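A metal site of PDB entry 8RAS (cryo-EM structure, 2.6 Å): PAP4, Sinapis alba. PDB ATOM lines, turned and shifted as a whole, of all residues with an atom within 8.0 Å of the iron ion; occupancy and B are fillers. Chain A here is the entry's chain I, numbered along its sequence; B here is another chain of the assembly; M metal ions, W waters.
The iron ion is bound by OD2 of Asp 211 (2.1 Å), water W1 (2.1 Å), NE2 of His 74 (2.3 Å) and NE2 of His 127 (2.5 Å).
The backbone carbonyl oxygen (O) of His 74 is in hydrogen-bond range of the backbone NH (N) of His 79, 2.9 Å away.
A ring nitrogen (ND1) of His 127 is in hydrogen-bond range of the backbone carbonyl oxygen (O) of Gln 123 (2.7 Å).
The indole nitrogen of Trp 176 sits at hydrogen-bond distance from the side-chain amide oxygen of Gln 123 (3.2 Å).
The backbone carbonyl oxygen (O) of His 127 lies close to the indole nitrogen (NE1) of Trp 131 (3.4 Å).
The side-chain carboxylate (OE1) of Glu 226 of chain B is in hydrogen-bond range of the backbone NH (N) of His 215, 2.8 Å away.
The side-chain carboxylate of Asp 211 sits close to the backbone NH of Trp 213 (3.1 Å).
A ring nitrogen (NE2) of His 78 lies close to a ring nitrogen (ND1) of His 215 (3.3 Å).
The backbone carbonyl oxygen of Asp 211 lies within hydrogen-bond range of the side-chain hydroxyl of Ser 216, 3.4 Å away.
Water W1 lies within hydrogen-bond range of a ring nitrogen (NE2) of His 215, the side-chain amide nitrogen of Gln 123 and the side-chain carboxylate of Asp 211.
Residues that only touch the iron ion: Trp 176 (3.7 Å) and His 215 (3.1 Å).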
ATOM      1  N   HIS A  74       4.561  11.946 -28.634  1.00  0.00           N
ATOM      2  CA  HIS A  74       3.201  12.294 -28.223  1.00  0.00           C
ATOM      3  C   HIS A  74       2.285  12.447 -29.422  1.00  0.00           C
ATOM      4  O   HIS A  74       1.069  12.229 -29.302  1.00  0.00           O
ATOM      5  CB  HIS A  74       3.219  13.578 -27.389  1.00  0.00           C
ATOM      6  CG  HIS A  74       2.045  13.727 -26.488  1.00  0.00           C
ATOM      7  ND1 HIS A  74       1.987  14.686 -25.494  1.00  0.00           N
ATOM      8  CD2 HIS A  74       0.873  13.055 -26.425  1.00  0.00           C
ATOM      9  CE1 HIS A  74       0.826  14.590 -24.859  1.00  0.00           C
ATOM     10  NE2 HIS A  74       0.135  13.609 -25.405  1.00  0.00           N
ATOM     11  N   TRP A  75       2.833  12.821 -30.580  1.00  0.00           N
ATOM     12  CA  TRP A  75       2.038  12.987 -31.793  1.00  0.00           C
ATOM     13  C   TRP A  75       2.371  11.976 -32.874  1.00  0.00           C
ATOM     14  O   TRP A  75       1.483  11.627 -33.654  1.00  0.00           O
ATOM     15  CB  TRP A  75       2.245  14.407 -32.357  1.00  0.00           C
ATOM     16  CG  TRP A  75       1.463  14.683 -33.599  1.00  0.00           C
ATOM     17  CD1 TRP A  75       0.146  15.045 -33.673  1.00  0.00           C
ATOM     18  CD2 TRP A  75       1.938  14.623 -34.951  1.00  0.00           C
ATOM     19  NE1 TRP A  75      -0.225  15.218 -34.983  1.00  0.00           N
ATOM     20  CE2 TRP A  75       0.860  14.967 -35.788  1.00  0.00           C
ATOM     21  CE3 TRP A  75       3.171  14.322 -35.531  1.00  0.00           C
ATOM     22  CZ2 TRP A  75       0.979  15.011 -37.176  1.00  0.00           C
ATOM     23  CZ3 TRP A  75       3.286  14.372 -36.907  1.00  0.00           C
ATOM     24  CH2 TRP A  75       2.192  14.709 -37.713  1.00  0.00           C
ATOM     25  N   HIS A  78       1.600   8.266 -30.256  1.00  0.00           N
ATOM     26  CA  HIS A  78       0.559   8.373 -29.234  1.00  0.00           C
ATOM     27  C   HIS A  78      -0.731   8.925 -29.829  1.00  0.00           C
ATOM     28  O   HIS A  78      -1.769   8.257 -29.829  1.00  0.00           O
ATOM     29  CB  HIS A  78       1.045   9.264 -28.085  1.00  0.00           C
ATOM     30  CG  HIS A  78       1.663   8.503 -26.957  1.00  0.00           C
ATOM     31  ND1 HIS A  78       1.052   7.437 -26.346  1.00  0.00           N
ATOM     32  CD2 HIS A  78       2.859   8.666 -26.331  1.00  0.00           C
ATOM     33  CE1 HIS A  78       1.837   6.973 -25.383  1.00  0.00           C
ATOM     34  NE2 HIS A  78       2.935   7.705 -25.352  1.00  0.00           N
ATOM     35  N   HIS A  79      -0.680  10.155 -30.344  1.00  0.00           N
ATOM     36  CA  HIS A  79      -1.886  10.757 -30.918  1.00  0.00           C
ATOM     37  C   HIS A  79      -2.279  10.084 -32.222  1.00  0.00           C
ATOM     38  O   HIS A  79      -3.473  10.005 -32.537  1.00  0.00           O
ATOM     39  CB  HIS A  79      -1.677  12.251 -31.126  1.00  0.00           C
ATOM     40  CG  HIS A  79      -2.902  12.976 -31.582  1.00  0.00           C
ATOM     41  ND1 HIS A  79      -4.160  12.424 -31.505  1.00  0.00           N
ATOM     42  CD2 HIS A  79      -3.068  14.214 -32.109  1.00  0.00           C
ATOM     43  CE1 HIS A  79      -5.047  13.286 -31.967  1.00  0.00           C
ATOM     44  NE2 HIS A  79      -4.409  14.381 -32.339  1.00  0.00           N
ATOM     45  N   TYR A  82      -4.177   6.734 -31.338  1.00  0.00           N
ATOM     46  CA  TYR A  82      -5.578   6.966 -30.994  1.00  0.00           C
ATOM     47  C   TYR A  82      -6.409   7.226 -32.245  1.00  0.00           C
ATOM     48  O   TYR A  82      -7.549   6.760 -32.353  1.00  0.00           O
ATOM     49  CB  TYR A  82      -5.685   8.142 -30.024  1.00  0.00           C
ATOM     50  CG  TYR A  82      -5.260   7.841 -28.615  1.00  0.00           C
ATOM     51  CD1 TYR A  82      -5.825   6.786 -27.904  1.00  0.00           C
ATOM     52  CD2 TYR A  82      -4.294   8.612 -27.973  1.00  0.00           C
ATOM     53  CE1 TYR A  82      -5.443   6.513 -26.611  1.00  0.00           C
ATOM     54  CE2 TYR A  82      -3.900   8.344 -26.686  1.00  0.00           C
ATOM     55  CZ  TYR A  82      -4.478   7.285 -26.002  1.00  0.00           C
ATOM     56  OH  TYR A  82      -4.092   7.022 -24.712  1.00  0.00           O
ATOM     57  N   GLN A 123      -9.824  10.589 -26.749  1.00  0.00           N
ATOM     58  CA  GLN A 123      -8.404  10.896 -26.631  1.00  0.00           C
ATOM     59  C   GLN A 123      -7.906  11.754 -27.786  1.00  0.00           C
ATOM     60  O   GLN A 123      -7.053  12.627 -27.591  1.00  0.00           O
ATOM     61  CB  GLN A 123      -7.588   9.614 -26.532  1.00  0.00           C
ATOM     62  CG  GLN A 123      -7.392   9.122 -25.106  1.00  0.00           C
ATOM     63  CD  GLN A 123      -6.615  10.096 -24.245  1.00  0.00           C
ATOM     64  OE1 GLN A 123      -7.197  10.959 -23.586  1.00  0.00           O
ATOM     65  NE2 GLN A 123      -5.303   9.960 -24.249  1.00  0.00           N
ATOM     66  N   ASN A 126      -8.887  15.385 -27.175  1.00  0.00           N
ATOM     67  CA  ASN A 126      -8.110  16.059 -26.148  1.00  0.00           C
ATOM     68  C   ASN A 126      -6.747  16.496 -26.681  1.00  0.00           C
ATOM     69  O   ASN A 126      -6.233  17.550 -26.283  1.00  0.00           O
ATOM     70  CB  ASN A 126      -7.946  15.132 -24.935  1.00  0.00           C
ATOM     71  CG  ASN A 126      -9.269  14.793 -24.287  1.00  0.00           C
ATOM     72  OD1 ASN A 126      -9.464  13.687 -23.786  1.00  0.00           O
ATOM     73  ND2 ASN A 126     -10.203  15.740 -24.316  1.00  0.00           N
ATOM     74  N   HIS A 127      -6.146  15.702 -27.567  1.00  0.00           N
ATOM     75  CA  HIS A 127      -4.807  16.008 -28.042  1.00  0.00           C
ATOM     76  C   HIS A 127      -4.802  17.219 -28.977  1.00  0.00           C
ATOM     77  O   HIS A 127      -3.966  18.110 -28.820  1.00  0.00           O
ATOM     78  CB  HIS A 127      -4.204  14.779 -28.726  1.00  0.00           C
ATOM     79  CG  HIS A 127      -3.669  13.766 -27.764  1.00  0.00           C
ATOM     80  ND1 HIS A 127      -4.484  12.974 -26.978  1.00  0.00           N
ATOM     81  CD2 HIS A 127      -2.398  13.422 -27.437  1.00  0.00           C
ATOM     82  CE1 HIS A 127      -3.739  12.192 -26.227  1.00  0.00           C
ATOM     83  NE2 HIS A 127      -2.476  12.439 -26.483  1.00  0.00           N
ATOM     84  N   PHE A 130      -5.151  19.937 -26.905  1.00  0.00           N
ATOM     85  CA  PHE A 130      -3.921  20.204 -26.185  1.00  0.00           C
ATOM     86  C   PHE A 130      -2.913  20.946 -27.054  1.00  0.00           C
ATOM     87  O   PHE A 130      -2.246  21.877 -26.591  1.00  0.00           O
ATOM     88  CB  PHE A 130      -3.311  18.900 -25.668  1.00  0.00           C
ATOM     89  CG  PHE A 130      -2.154  19.102 -24.741  1.00  0.00           C
ATOM     90  CD1 PHE A 130      -2.245  19.965 -23.666  1.00  0.00           C
ATOM     91  CD2 PHE A 130      -0.964  18.418 -24.937  1.00  0.00           C
ATOM     92  CE1 PHE A 130      -1.174  20.148 -22.808  1.00  0.00           C
ATOM     93  CE2 PHE A 130       0.099  18.592 -24.085  1.00  0.00           C
ATOM     94  CZ  PHE A 130      -0.004  19.458 -23.017  1.00  0.00           C
ATOM     95  N   TRP A 131      -2.781  20.548 -28.322  1.00  0.00           N
ATOM     96  CA  TRP A 131      -1.828  21.205 -29.211  1.00  0.00           C
ATOM     97  C   TRP A 131      -2.185  22.670 -29.409  1.00  0.00           C
ATOM     98  O   TRP A 131      -1.309  23.543 -29.368  1.00  0.00           O
ATOM     99  CB  TRP A 131      -1.754  20.484 -30.548  1.00  0.00           C
ATOM    100  CG  TRP A 131      -1.495  18.999 -30.480  1.00  0.00           C
ATOM    101  CD1 TRP A 131      -2.123  18.025 -31.210  1.00  0.00           C
ATOM    102  CD2 TRP A 131      -0.545  18.327 -29.637  1.00  0.00           C
ATOM    103  NE1 TRP A 131      -1.621  16.790 -30.873  1.00  0.00           N
ATOM    104  CE2 TRP A 131      -0.658  16.948 -29.918  1.00  0.00           C
ATOM    105  CE3 TRP A 131       0.389  18.744 -28.686  1.00  0.00           C
ATOM    106  CZ2 TRP A 131       0.129  15.990 -29.277  1.00  0.00           C
ATOM    107  CZ3 TRP A 131       1.154  17.794 -28.048  1.00  0.00           C
ATOM    108  CH2 TRP A 131       1.024  16.440 -28.345  1.00  0.00           C
ATOM    109  N   GLY A 175      -4.389  11.556 -16.514  1.00  0.00           N
ATOM    110  CA  GLY A 175      -5.629  12.282 -16.620  1.00  0.00           C
ATOM    111  C   GLY A 175      -5.437  13.613 -17.311  1.00  0.00           C
ATOM    112  O   GLY A 175      -4.453  13.816 -18.020  1.00  0.00           O
ATOM    113  N   TRP A 176      -6.394  14.510 -17.091  1.00  0.00           N
ATOM    114  CA  TRP A 176      -6.344  15.834 -17.705  1.00  0.00           C
ATOM    115  C   TRP A 176      -6.793  16.884 -16.696  1.00  0.00           C
ATOM    116  O   TRP A 176      -7.505  16.589 -15.726  1.00  0.00           O
ATOM    117  CB  TRP A 176      -7.229  15.904 -18.954  1.00  0.00           C
ATOM    118  CG  TRP A 176      -6.880  14.896 -19.999  1.00  0.00           C
ATOM    119  CD1 TRP A 176      -7.254  13.589 -20.035  1.00  0.00           C
ATOM    120  CD2 TRP A 176      -6.094  15.121 -21.172  1.00  0.00           C
ATOM    121  NE1 TRP A 176      -6.740  12.985 -21.156  1.00  0.00           N
ATOM    122  CE2 TRP A 176      -6.027  13.897 -21.875  1.00  0.00           C
ATOM    123  CE3 TRP A 176      -5.439  16.236 -21.710  1.00  0.00           C
ATOM    124  CZ2 TRP A 176      -5.335  13.769 -23.076  1.00  0.00           C
ATOM    125  CZ3 TRP A 176      -4.755  16.105 -22.896  1.00  0.00           C
ATOM    126  CH2 TRP A 176      -4.703  14.874 -23.569  1.00  0.00           C
ATOM    127  N   ASN A 209      -6.312  23.467 -22.004  1.00  0.00           N
ATOM    128  CA  ASN A 209      -6.038  22.048 -21.806  1.00  0.00           C
ATOM    129  C   ASN A 209      -4.619  21.858 -21.288  1.00  0.00           C
ATOM    130  O   ASN A 209      -3.685  22.519 -21.749  1.00  0.00           O
ATOM    131  CB  ASN A 209      -6.215  21.270 -23.120  1.00  0.00           C
ATOM    132  CG  ASN A 209      -6.224  19.770 -22.916  1.00  0.00           C
ATOM    133  OD1 ASN A 209      -5.430  19.228 -22.159  1.00  0.00           O
ATOM    134  ND2 ASN A 209      -7.135  19.087 -23.603  1.00  0.00           N
ATOM    135  N   LEU A 210      -4.475  20.943 -20.322  1.00  0.00           N
ATOM    136  CA  LEU A 210      -3.170  20.506 -19.846  1.00  0.00           C
ATOM    137  C   LEU A 210      -3.196  18.989 -19.720  1.00  0.00           C
ATOM    138  O   LEU A 210      -4.144  18.431 -19.165  1.00  0.00           O
ATOM    139  CB  LEU A 210      -2.812  21.150 -18.500  1.00  0.00           C
ATOM    140  CG  LEU A 210      -1.531  20.645 -17.840  1.00  0.00           C
ATOM    141  CD1 LEU A 210      -0.334  20.745 -18.780  1.00  0.00           C
ATOM    142  CD2 LEU A 210      -1.251  21.406 -16.548  1.00  0.00           C
ATOM    143  N   ASP A 211      -2.153  18.336 -20.239  1.00  0.00           N
ATOM    144  CA  ASP A 211      -2.039  16.885 -20.185  1.00  0.00           C
ATOM    145  C   ASP A 211      -1.111  16.506 -19.043  1.00  0.00           C
ATOM    146  O   ASP A 211       0.060  16.882 -19.039  1.00  0.00           O
ATOM    147  CB  ASP A 211      -1.505  16.334 -21.510  1.00  0.00           C
ATOM    148  CG  ASP A 211      -1.769  14.853 -21.666  1.00  0.00           C
ATOM    149  OD1 ASP A 211      -2.385  14.251 -20.761  1.00  0.00           O
ATOM    150  OD2 ASP A 211      -1.365  14.276 -22.706  1.00  0.00           O
ATOM    151  N   VAL A 212      -1.640  15.758 -18.085  1.00  0.00           N
ATOM    152  CA  VAL A 212      -0.847  15.245 -16.977  1.00  0.00           C
ATOM    153  C   VAL A 212      -0.602  13.741 -17.099  1.00  0.00           C
ATOM    154  O   VAL A 212      -0.198  13.102 -16.129  1.00  0.00           O
ATOM    155  CB  VAL A 212      -1.479  15.588 -15.617  1.00  0.00           C
ATOM    156  CG1 VAL A 212      -1.394  17.086 -15.358  1.00  0.00           C
ATOM    157  CG2 VAL A 212      -2.906  15.106 -15.546  1.00  0.00           C
ATOM    158  N   TRP A 213      -0.866  13.167 -18.274  1.00  0.00           N
ATOM    159  CA  TRP A 213      -0.425  11.804 -18.547  1.00  0.00           C
ATOM    160  C   TRP A 213       1.091  11.734 -18.464  1.00  0.00           C
ATOM    161  O   TRP A 213       1.791  12.658 -18.901  1.00  0.00           O
ATOM    162  CB  TRP A 213      -0.900  11.346 -19.926  1.00  0.00           C
ATOM    163  CG  TRP A 213      -2.325  10.862 -19.967  1.00  0.00           C
ATOM    164  CD1 TRP A 213      -3.441  11.565 -19.608  1.00  0.00           C
ATOM    165  CD2 TRP A 213      -2.784   9.589 -20.411  1.00  0.00           C
ATOM    166  NE1 TRP A 213      -4.559  10.795 -19.792  1.00  0.00           N
ATOM    167  CE2 TRP A 213      -4.187   9.576 -20.282  1.00  0.00           C
ATOM    168  CE3 TRP A 213      -2.144   8.439 -20.898  1.00  0.00           C
ATOM    169  CZ2 TRP A 213      -4.961   8.476 -20.632  1.00  0.00           C
ATOM    170  CZ3 TRP A 213      -2.922   7.344 -21.236  1.00  0.00           C
ATOM    171  CH2 TRP A 213      -4.314   7.372 -21.106  1.00  0.00           C
ATOM    172  N   GLU A 214       1.603  10.642 -17.903  1.00  0.00           N
ATOM    173  CA  GLU A 214       3.036  10.522 -17.687  1.00  0.00           C
ATOM    174  C   GLU A 214       3.801  10.589 -19.000  1.00  0.00           C
ATOM    175  O   GLU A 214       4.851  11.235 -19.091  1.00  0.00           O
ATOM    176  CB  GLU A 214       3.350   9.234 -16.936  1.00  0.00           C
ATOM    177  CG  GLU A 214       3.008   9.289 -15.456  1.00  0.00           C
ATOM    178  CD  GLU A 214       3.418   8.034 -14.719  1.00  0.00           C
ATOM    179  OE1 GLU A 214       3.384   6.951 -15.324  1.00  0.00           O
ATOM    180  OE2 GLU A 214       3.786   8.143 -13.528  1.00  0.00           O
ATOM    181  N   HIS A 215       3.280   9.935 -20.048  1.00  0.00           N
ATOM    182  CA  HIS A 215       3.958   9.911 -21.332  1.00  0.00           C
ATOM    183  C   HIS A 215       4.121  11.303 -21.939  1.00  0.00           C
ATOM    184  O   HIS A 215       4.968  11.490 -22.816  1.00  0.00           O
ATOM    185  CB  HIS A 215       3.206   9.004 -22.312  1.00  0.00           C
ATOM    186  CG  HIS A 215       1.924   9.584 -22.804  1.00  0.00           C
ATOM    187  ND1 HIS A 215       1.851  10.417 -23.903  1.00  0.00           N
ATOM    188  CD2 HIS A 215       0.648   9.443 -22.365  1.00  0.00           C
ATOM    189  CE1 HIS A 215       0.598  10.769 -24.106  1.00  0.00           C
ATOM    190  NE2 HIS A 215      -0.154  10.194 -23.186  1.00  0.00           N
ATOM    191  N   SER A 216       3.335  12.278 -21.486  1.00  0.00           N
ATOM    192  CA  SER A 216       3.431  13.623 -22.046  1.00  0.00           C
ATOM    193  C   SER A 216       4.665  14.358 -21.557  1.00  0.00           C
ATOM    194  O   SER A 216       5.197  15.214 -22.263  1.00  0.00           O
ATOM    195  CB  SER A 216       2.165  14.417 -21.705  1.00  0.00           C
ATOM    196  OG  SER A 216       1.886  14.371 -20.321  1.00  0.00           O
ATOM    197  N   TYR A 217       5.142  14.046 -20.336  1.00  0.00           N
ATOM    198  CA  TYR A 217       6.233  14.810 -19.763  1.00  0.00           C
ATOM    199  C   TYR A 217       7.271  13.942 -19.038  1.00  0.00           C
ATOM    200  O   TYR A 217       8.011  14.463 -18.198  1.00  0.00           O
ATOM    201  CB  TYR A 217       5.689  15.859 -18.777  1.00  0.00           C
ATOM    202  CG  TYR A 217       4.954  15.277 -17.598  1.00  0.00           C
ATOM    203  CD1 TYR A 217       3.613  14.922 -17.692  1.00  0.00           C
ATOM    204  CD2 TYR A 217       5.602  15.084 -16.381  1.00  0.00           C
ATOM    205  CE1 TYR A 217       2.944  14.383 -16.615  1.00  0.00           C
ATOM    206  CE2 TYR A 217       4.924  14.549 -15.300  1.00  0.00           C
ATOM    207  CZ  TYR A 217       3.603  14.201 -15.415  1.00  0.00           C
ATOM    208  OH  TYR A 217       2.934  13.662 -14.338  1.00  0.00           O
ATOM    209  N   GLU B 226       3.087   4.219 -17.151  1.00  0.00           N
ATOM    210  CA  GLU B 226       4.052   4.617 -18.172  1.00  0.00           C
ATOM    211  C   GLU B 226       5.408   4.962 -17.574  1.00  0.00           C
ATOM    212  O   GLU B 226       6.438   4.806 -18.254  1.00  0.00           O
ATOM    213  CB  GLU B 226       3.497   5.788 -18.976  1.00  0.00           C
ATOM    214  CG  GLU B 226       2.240   5.447 -19.753  1.00  0.00           C
ATOM    215  CD  GLU B 226       1.604   6.651 -20.413  1.00  0.00           C
ATOM    216  OE1 GLU B 226       1.573   7.726 -19.778  1.00  0.00           O
ATOM    217  OE2 GLU B 226       1.148   6.526 -21.562  1.00  0.00           O
HETATM  218 FE    FE M   1      -1.706  12.874 -24.186  1.00  0.00          FE
HETATM  219  O   HOH W   1      -2.907  11.650 -22.908  1.00  0.00           O
